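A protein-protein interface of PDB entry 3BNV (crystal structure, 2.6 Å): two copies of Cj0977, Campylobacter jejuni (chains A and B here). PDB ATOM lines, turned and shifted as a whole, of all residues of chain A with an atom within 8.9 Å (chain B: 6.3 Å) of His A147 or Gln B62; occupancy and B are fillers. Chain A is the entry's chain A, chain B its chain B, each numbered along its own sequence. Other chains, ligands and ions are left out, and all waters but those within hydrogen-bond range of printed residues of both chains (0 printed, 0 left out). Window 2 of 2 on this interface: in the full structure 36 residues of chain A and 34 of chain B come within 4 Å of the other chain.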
ATOM      1  N   PRO A  29       9.863  12.146 -13.455  1.00  0.00           N
ATOM      2  CA  PRO A  29      10.798  13.263 -13.558  1.00  0.00           C
ATOM      3  C   PRO A  29      11.308  13.708 -12.198  1.00  0.00           C
ATOM      4  O   PRO A  29      12.365  14.356 -12.104  1.00  0.00           O
ATOM      5  CB  PRO A  29       9.947  14.380 -14.175  1.00  0.00           C
ATOM      6  CG  PRO A  29       8.521  13.958 -13.940  1.00  0.00           C
ATOM      7  CD  PRO A  29       8.510  12.480 -13.933  1.00  0.00           C
ATOM      8  N   GLU A  30      10.566  13.368 -11.149  1.00  0.00           N
ATOM      9  CA  GLU A  30      10.806  13.982  -9.854  1.00  0.00           C
ATOM     10  C   GLU A  30      11.374  12.989  -8.867  1.00  0.00           C
ATOM     11  O   GLU A  30      11.577  13.309  -7.707  1.00  0.00           O
ATOM     12  CB  GLU A  30       9.487  14.547  -9.342  1.00  0.00           C
ATOM     13  CG  GLU A  30       9.657  15.602  -8.319  1.00  0.00           C
ATOM     14  CD  GLU A  30      10.023  16.936  -8.926  1.00  0.00           C
ATOM     15  OE1 GLU A  30      10.562  16.958 -10.056  1.00  0.00           O
ATOM     16  OE2 GLU A  30       9.764  17.961  -8.266  1.00  0.00           O
ATOM     17  N   GLU A  85       5.277   9.646 -20.542  1.00  0.00           N
ATOM     18  CA  GLU A  85       5.164  10.683 -19.542  1.00  0.00           C
ATOM     19  C   GLU A  85       4.232  10.272 -18.417  1.00  0.00           C
ATOM     20  O   GLU A  85       4.474  10.586 -17.270  1.00  0.00           O
ATOM     21  CB  GLU A  85       4.685  11.990 -20.150  1.00  0.00           C
ATOM     22  CG  GLU A  85       4.593  13.102 -19.128  1.00  0.00           C
ATOM     23  CD  GLU A  85       4.343  14.426 -19.763  1.00  0.00           C
ATOM     24  OE1 GLU A  85       4.575  15.461 -19.091  1.00  0.00           O
ATOM     25  OE2 GLU A  85       3.915  14.423 -20.941  1.00  0.00           O
ATOM     26  N   PHE A  86       3.154   9.582 -18.748  1.00  0.00           N
ATOM     27  CA  PHE A  86       2.180   9.182 -17.746  1.00  0.00           C
ATOM     28  C   PHE A  86       2.068   7.662 -17.659  1.00  0.00           C
ATOM     29  O   PHE A  86       1.359   7.042 -18.436  1.00  0.00           O
ATOM     30  CB  PHE A  86       0.801   9.778 -18.058  1.00  0.00           C
ATOM     31  CG  PHE A  86       0.805  11.263 -18.287  1.00  0.00           C
ATOM     32  CD1 PHE A  86       0.393  11.787 -19.510  1.00  0.00           C
ATOM     33  CD2 PHE A  86       1.176  12.139 -17.273  1.00  0.00           C
ATOM     34  CE1 PHE A  86       0.367  13.157 -19.731  1.00  0.00           C
ATOM     35  CE2 PHE A  86       1.161  13.499 -17.476  1.00  0.00           C
ATOM     36  CZ  PHE A  86       0.758  14.020 -18.709  1.00  0.00           C
ATOM     37  N   SER A  87       2.753   7.062 -16.699  1.00  0.00           N
ATOM     38  CA  SER A  87       2.705   5.626 -16.543  1.00  0.00           C
ATOM     39  C   SER A  87       2.802   5.252 -15.079  1.00  0.00           C
ATOM     40  O   SER A  87       3.240   6.044 -14.246  1.00  0.00           O
ATOM     41  CB  SER A  87       3.826   4.955 -17.328  1.00  0.00           C
ATOM     42  OG  SER A  87       5.055   5.204 -16.705  1.00  0.00           O
ATOM     43  N   VAL A  88       2.371   4.039 -14.776  1.00  0.00           N
ATOM     44  CA  VAL A  88       2.521   3.496 -13.454  1.00  0.00           C
ATOM     45  C   VAL A  88       2.797   2.027 -13.612  1.00  0.00           C
ATOM     46  O   VAL A  88       2.676   1.483 -14.731  1.00  0.00           O
ATOM     47  CB  VAL A  88       1.260   3.708 -12.591  1.00  0.00           C
ATOM     48  CG1 VAL A  88       0.874   5.166 -12.560  1.00  0.00           C
ATOM     49  CG2 VAL A  88       0.106   2.851 -13.079  1.00  0.00           C
ATOM     50  N   SER A 143       0.383   2.784 -19.336  1.00  0.00           N
ATOM     51  CA  SER A 143       0.454   4.227 -19.558  1.00  0.00           C
ATOM     52  C   SER A 143      -0.882   4.832 -19.946  1.00  0.00           C
ATOM     53  O   SER A 143      -1.819   4.143 -20.367  1.00  0.00           O
ATOM     54  CB  SER A 143       1.550   4.601 -20.560  1.00  0.00           C
ATOM     55  OG  SER A 143       1.381   3.940 -21.795  1.00  0.00           O
ATOM     56  N   THR A 144      -0.999   6.130 -19.757  1.00  0.00           N
ATOM     57  CA  THR A 144      -2.213   6.779 -20.174  1.00  0.00           C
ATOM     58  C   THR A 144      -1.848   8.012 -20.986  1.00  0.00           C
ATOM     59  O   THR A 144      -0.683   8.446 -20.985  1.00  0.00           O
ATOM     60  CB  THR A 144      -3.119   7.082 -18.966  1.00  0.00           C
ATOM     61  OG1 THR A 144      -2.355   7.738 -17.944  1.00  0.00           O
ATOM     62  CG2 THR A 144      -3.666   5.780 -18.387  1.00  0.00           C
ATOM     63  N   ASP A 145      -2.822   8.550 -21.715  1.00  0.00           N
ATOM     64  CA  ASP A 145      -2.565   9.729 -22.544  1.00  0.00           C
ATOM     65  C   ASP A 145      -2.584  10.959 -21.654  1.00  0.00           C
ATOM     66  O   ASP A 145      -1.962  11.967 -21.976  1.00  0.00           O
ATOM     67  CB  ASP A 145      -3.563   9.858 -23.711  1.00  0.00           C
ATOM     68  CG  ASP A 145      -3.715   8.558 -24.511  1.00  0.00           C
ATOM     69  OD1 ASP A 145      -4.095   7.534 -23.899  1.00  0.00           O
ATOM     70  OD2 ASP A 145      -3.475   8.551 -25.743  1.00  0.00           O
ATOM     71  N   GLU A 146      -3.268  10.856 -20.512  1.00  0.00           N
ATOM     72  CA  GLU A 146      -3.252  11.920 -19.498  1.00  0.00           C
ATOM     73  C   GLU A 146      -2.835  11.425 -18.113  1.00  0.00           C
ATOM     74  O   GLU A 146      -2.827  10.228 -17.854  1.00  0.00           O
ATOM     75  CB  GLU A 146      -4.598  12.645 -19.450  1.00  0.00           C
ATOM     76  CG  GLU A 146      -4.794  13.552 -20.658  1.00  0.00           C
ATOM     77  CD  GLU A 146      -6.259  13.858 -20.974  1.00  0.00           C
ATOM     78  OE1 GLU A 146      -7.092  13.989 -20.036  1.00  0.00           O
ATOM     79  OE2 GLU A 146      -6.569  13.989 -22.184  1.00  0.00           O
ATOM     80  N   HIS A 147      -2.472  12.347 -17.226  1.00  0.00           N
ATOM     81  CA  HIS A 147      -2.026  11.948 -15.905  1.00  0.00           C
ATOM     82  C   HIS A 147      -3.119  11.215 -15.177  1.00  0.00           C
ATOM     83  O   HIS A 147      -4.272  11.644 -15.203  1.00  0.00           O
ATOM     84  CB  HIS A 147      -1.589  13.137 -15.068  1.00  0.00           C
ATOM     85  CG  HIS A 147      -0.915  12.730 -13.802  1.00  0.00           C
ATOM     86  ND1 HIS A 147      -1.616  12.372 -12.674  1.00  0.00           N
ATOM     87  CD2 HIS A 147       0.391  12.538 -13.512  1.00  0.00           C
ATOM     88  CE1 HIS A 147      -0.770  12.001 -11.732  1.00  0.00           C
ATOM     89  NE2 HIS A 147       0.457  12.093 -12.214  1.00  0.00           N
ATOM     90  N   ILE A 148      -2.765  10.135 -14.492  1.00  0.00           N
ATOM     91  CA  ILE A 148      -3.780   9.273 -13.886  1.00  0.00           C
ATOM     92  C   ILE A 148      -4.783   9.960 -12.947  1.00  0.00           C
ATOM     93  O   ILE A 148      -5.941   9.572 -12.923  1.00  0.00           O
ATOM     94  CB  ILE A 148      -3.169   7.983 -13.233  1.00  0.00           C
ATOM     95  CG1 ILE A 148      -4.267   6.950 -12.943  1.00  0.00           C
ATOM     96  CG2 ILE A 148      -2.357   8.302 -11.978  1.00  0.00           C
ATOM     97  CD1 ILE A 148      -3.760   5.510 -12.940  1.00  0.00           C
ATOM     98  N   PHE A 149      -4.364  10.980 -12.202  1.00  0.00           N
ATOM     99  CA  PHE A 149      -5.247  11.598 -11.215  1.00  0.00           C
ATOM    100  C   PHE A 149      -6.215  12.593 -11.839  1.00  0.00           C
ATOM    101  O   PHE A 149      -7.007  13.234 -11.129  1.00  0.00           O
ATOM    102  CB  PHE A 149      -4.444  12.308 -10.117  1.00  0.00           C
ATOM    103  CG  PHE A 149      -3.651  11.376  -9.236  1.00  0.00           C
ATOM    104  CD1 PHE A 149      -2.434  11.777  -8.698  1.00  0.00           C
ATOM    105  CD2 PHE A 149      -4.121  10.104  -8.944  1.00  0.00           C
ATOM    106  CE1 PHE A 149      -1.698  10.918  -7.886  1.00  0.00           C
ATOM    107  CE2 PHE A 149      -3.391   9.246  -8.127  1.00  0.00           C
ATOM    108  CZ  PHE A 149      -2.178   9.652  -7.610  1.00  0.00           C
ATOM    109  N   LYS A 150      -6.153  12.725 -13.165  1.00  0.00           N
ATOM    110  CA  LYS A 150      -6.925  13.739 -13.884  1.00  0.00           C
ATOM    111  C   LYS A 150      -7.976  13.095 -14.785  1.00  0.00           C
ATOM    112  O   LYS A 150      -8.258  11.903 -14.658  1.00  0.00           O
ATOM    113  CB  LYS A 150      -5.979  14.642 -14.694  1.00  0.00           C
ATOM    114  CG  LYS A 150      -6.537  15.168 -16.031  1.00  0.00           C
ATOM    115  CD  LYS A 150      -5.502  16.056 -16.751  1.00  0.00           C
ATOM    116  CE  LYS A 150      -6.130  16.916 -17.873  1.00  0.00           C
ATOM    117  NZ  LYS A 150      -5.775  16.475 -19.267  1.00  0.00           N
ATOM    118  N   ASP B  60       6.508  12.486  -9.378  1.00  0.00           N
ATOM    119  CA  ASP B  60       6.293  13.684 -10.187  1.00  0.00           C
ATOM    120  C   ASP B  60       5.840  14.868  -9.365  1.00  0.00           C
ATOM    121  O   ASP B  60       5.725  14.765  -8.151  1.00  0.00           O
ATOM    122  CB  ASP B  60       5.323  13.437 -11.359  1.00  0.00           C
ATOM    123  CG  ASP B  60       3.933  12.980 -10.910  1.00  0.00           C
ATOM    124  OD1 ASP B  60       3.285  12.254 -11.701  1.00  0.00           O
ATOM    125  OD2 ASP B  60       3.492  13.342  -9.791  1.00  0.00           O
ATOM    126  N   ASP B  61       5.581  15.996 -10.018  1.00  0.00           N
ATOM    127  CA  ASP B  61       5.152  17.183  -9.292  1.00  0.00           C
ATOM    128  C   ASP B  61       3.633  17.243  -9.138  1.00  0.00           C
ATOM    129  O   ASP B  61       3.099  18.272  -8.761  1.00  0.00           O
ATOM    130  CB  ASP B  61       5.683  18.462  -9.949  1.00  0.00           C
ATOM    131  CG  ASP B  61       4.793  18.960 -11.079  1.00  0.00           C
ATOM    132  OD1 ASP B  61       4.340  18.123 -11.903  1.00  0.00           O
ATOM    133  OD2 ASP B  61       4.544  20.189 -11.142  1.00  0.00           O
ATOM    134  N   GLN B  62       2.944  16.135  -9.416  1.00  0.00           N
ATOM    135  CA  GLN B  62       1.490  16.064  -9.230  1.00  0.00           C
ATOM    136  C   GLN B  62       1.109  15.273  -7.987  1.00  0.00           C
ATOM    137  O   GLN B  62      -0.078  15.081  -7.729  1.00  0.00           O
ATOM    138  CB  GLN B  62       0.784  15.435 -10.438  1.00  0.00           C
ATOM    139  CG  GLN B  62       1.130  16.038 -11.777  1.00  0.00           C
ATOM    140  CD  GLN B  62       0.523  17.392 -11.956  1.00  0.00           C
ATOM    141  OE1 GLN B  62      -0.500  17.536 -12.632  1.00  0.00           O
ATOM    142  NE2 GLN B  62       1.125  18.400 -11.340  1.00  0.00           N
ATOM    143  N   GLY B  63       2.100  14.796  -7.232  1.00  0.00           N
ATOM    144  CA  GLY B  63       1.822  14.080  -5.992  1.00  0.00           C
ATOM    145  C   GLY B  63       1.732  12.574  -6.151  1.00  0.00           C
ATOM    146  O   GLY B  63       1.360  11.866  -5.215  1.00  0.00           O
ATOM    147  N   LEU B  64       2.076  12.078  -7.332  1.00  0.00           N
ATOM    148  CA  LEU B  64       2.057  10.641  -7.573  1.00  0.00           C
ATOM    149  C   LEU B  64       3.185   9.965  -6.803  1.00  0.00           C
ATOM    150  O   LEU B  64       4.334  10.398  -6.854  1.00  0.00           O
ATOM    151  CB  LEU B  64       2.180  10.353  -9.075  1.00  0.00           C
ATOM    152  CG  LEU B  64       2.212   8.920  -9.614  1.00  0.00           C
ATOM    153  CD1 LEU B  64       0.887   8.293  -9.408  1.00  0.00           C
ATOM    154  CD2 LEU B  64       2.525   8.934 -11.075  1.00  0.00           C
ATOM    155  N   LYS B 101      -1.513   8.742  -3.655  1.00  0.00           N
ATOM    156  CA  LYS B 101      -1.304  10.160  -3.862  1.00  0.00           C
ATOM    157  C   LYS B 101      -0.736  10.791  -2.593  1.00  0.00           C
ATOM    158  O   LYS B 101      -1.124  10.433  -1.484  1.00  0.00           O
ATOM    159  CB  LYS B 101      -2.611  10.845  -4.255  1.00  0.00           C
ATOM    160  CG  LYS B 101      -2.563  12.363  -4.120  1.00  0.00           C
ATOM    161  CD  LYS B 101      -3.366  13.083  -5.198  1.00  0.00           C
ATOM    162  CE  LYS B 101      -3.264  14.609  -5.018  1.00  0.00           C
ATOM    163  NZ  LYS B 101      -3.529  15.394  -6.266  1.00  0.00           N
ATOM    164  N   LEU B 102       0.189  11.731  -2.754  1.00  0.00           N
ATOM    165  CA  LEU B 102       0.791  12.382  -1.615  1.00  0.00           C
ATOM    166  C   LEU B 102      -0.290  12.829  -0.655  1.00  0.00           C
ATOM    167  O   LEU B 102      -1.260  13.472  -1.056  1.00  0.00           O
ATOM    168  CB  LEU B 102       1.576  13.598  -2.058  1.00  0.00           C
ATOM    169  CG  LEU B 102       2.845  13.884  -1.255  1.00  0.00           C
ATOM    170  CD1 LEU B 102       2.978  15.371  -1.008  1.00  0.00           C
ATOM    171  CD2 LEU B 102       2.881  13.110   0.064  1.00  0.00           C
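NE2 of His A147 is in hydrogen-bond range of OD1 of Asp B60 (2.9 Å).
A ring nitrogen (ND1) of His A147 is in hydrogen-bond range of the backbone NH (N) of Phe A149 (3.1 Å). The side-chain carboxylate (OD2) of Asp B60 sits at hydrogen-bond distance from the backbone NH (N) of Gln B62. The side-chain carboxylate of Asp B60 lies within hydrogen-bond range of the backbone NH of Gly B63 (3.3 Å). N of Leu B64 is in hydrogen-bond range of OD2 of Asp B60 (3.1 Å). The side-chain amide nitrogen (NE2) of Gln B62 is in hydrogen-bond range of the side-chain carboxylate (OD1) of Asp B61 (3.3 Å).
Asp B60 touches Glu A30. NE2 of His A147 touches CB of Gln B62, 3.8 Å away. His A147 touches Leu B64. Leu B64 touches Phe A149. CZ of Phe A149 touches CB of Lys B101, 3.6 Å away.
His A147 touches three residues of chain B. Gln B62 touches one residue of chain A. Of the printed residues of chain B, Phe A149 touches Leu B64 (3.8 Å) and Lys B101 (3.6 Å). Of the printed residues of chain A, Asp B60 touches Glu A30 (3.4 Å) and His A147 (2.9 Å). The nearest residue of chain B that does not touch His A147 is Gly B63 (5.9 Å). The nearest residue of chain A that does not touch Gln B62 is Phe A149 (4.2 Å). The nearest printed residue of chain B that does not touch Glu A30 is Asp B61 (4.2 Å).
Printed residues of chain A that touch a printed residue of chain B: Glu A30, His A147 and Phe A149. Of the 7 printed residues of chain B, 4 touch a printed residue of chain A. Hydrophobic or aromatic side chains of chain B within 4 Å of the printed part of chain A: Leu B64. Along chain B the printed residues that touch a printed residue of chain A span positions 60 to 101. Among the printed residues, 6 pairs touch across the chains.
No position is printed for both chains.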
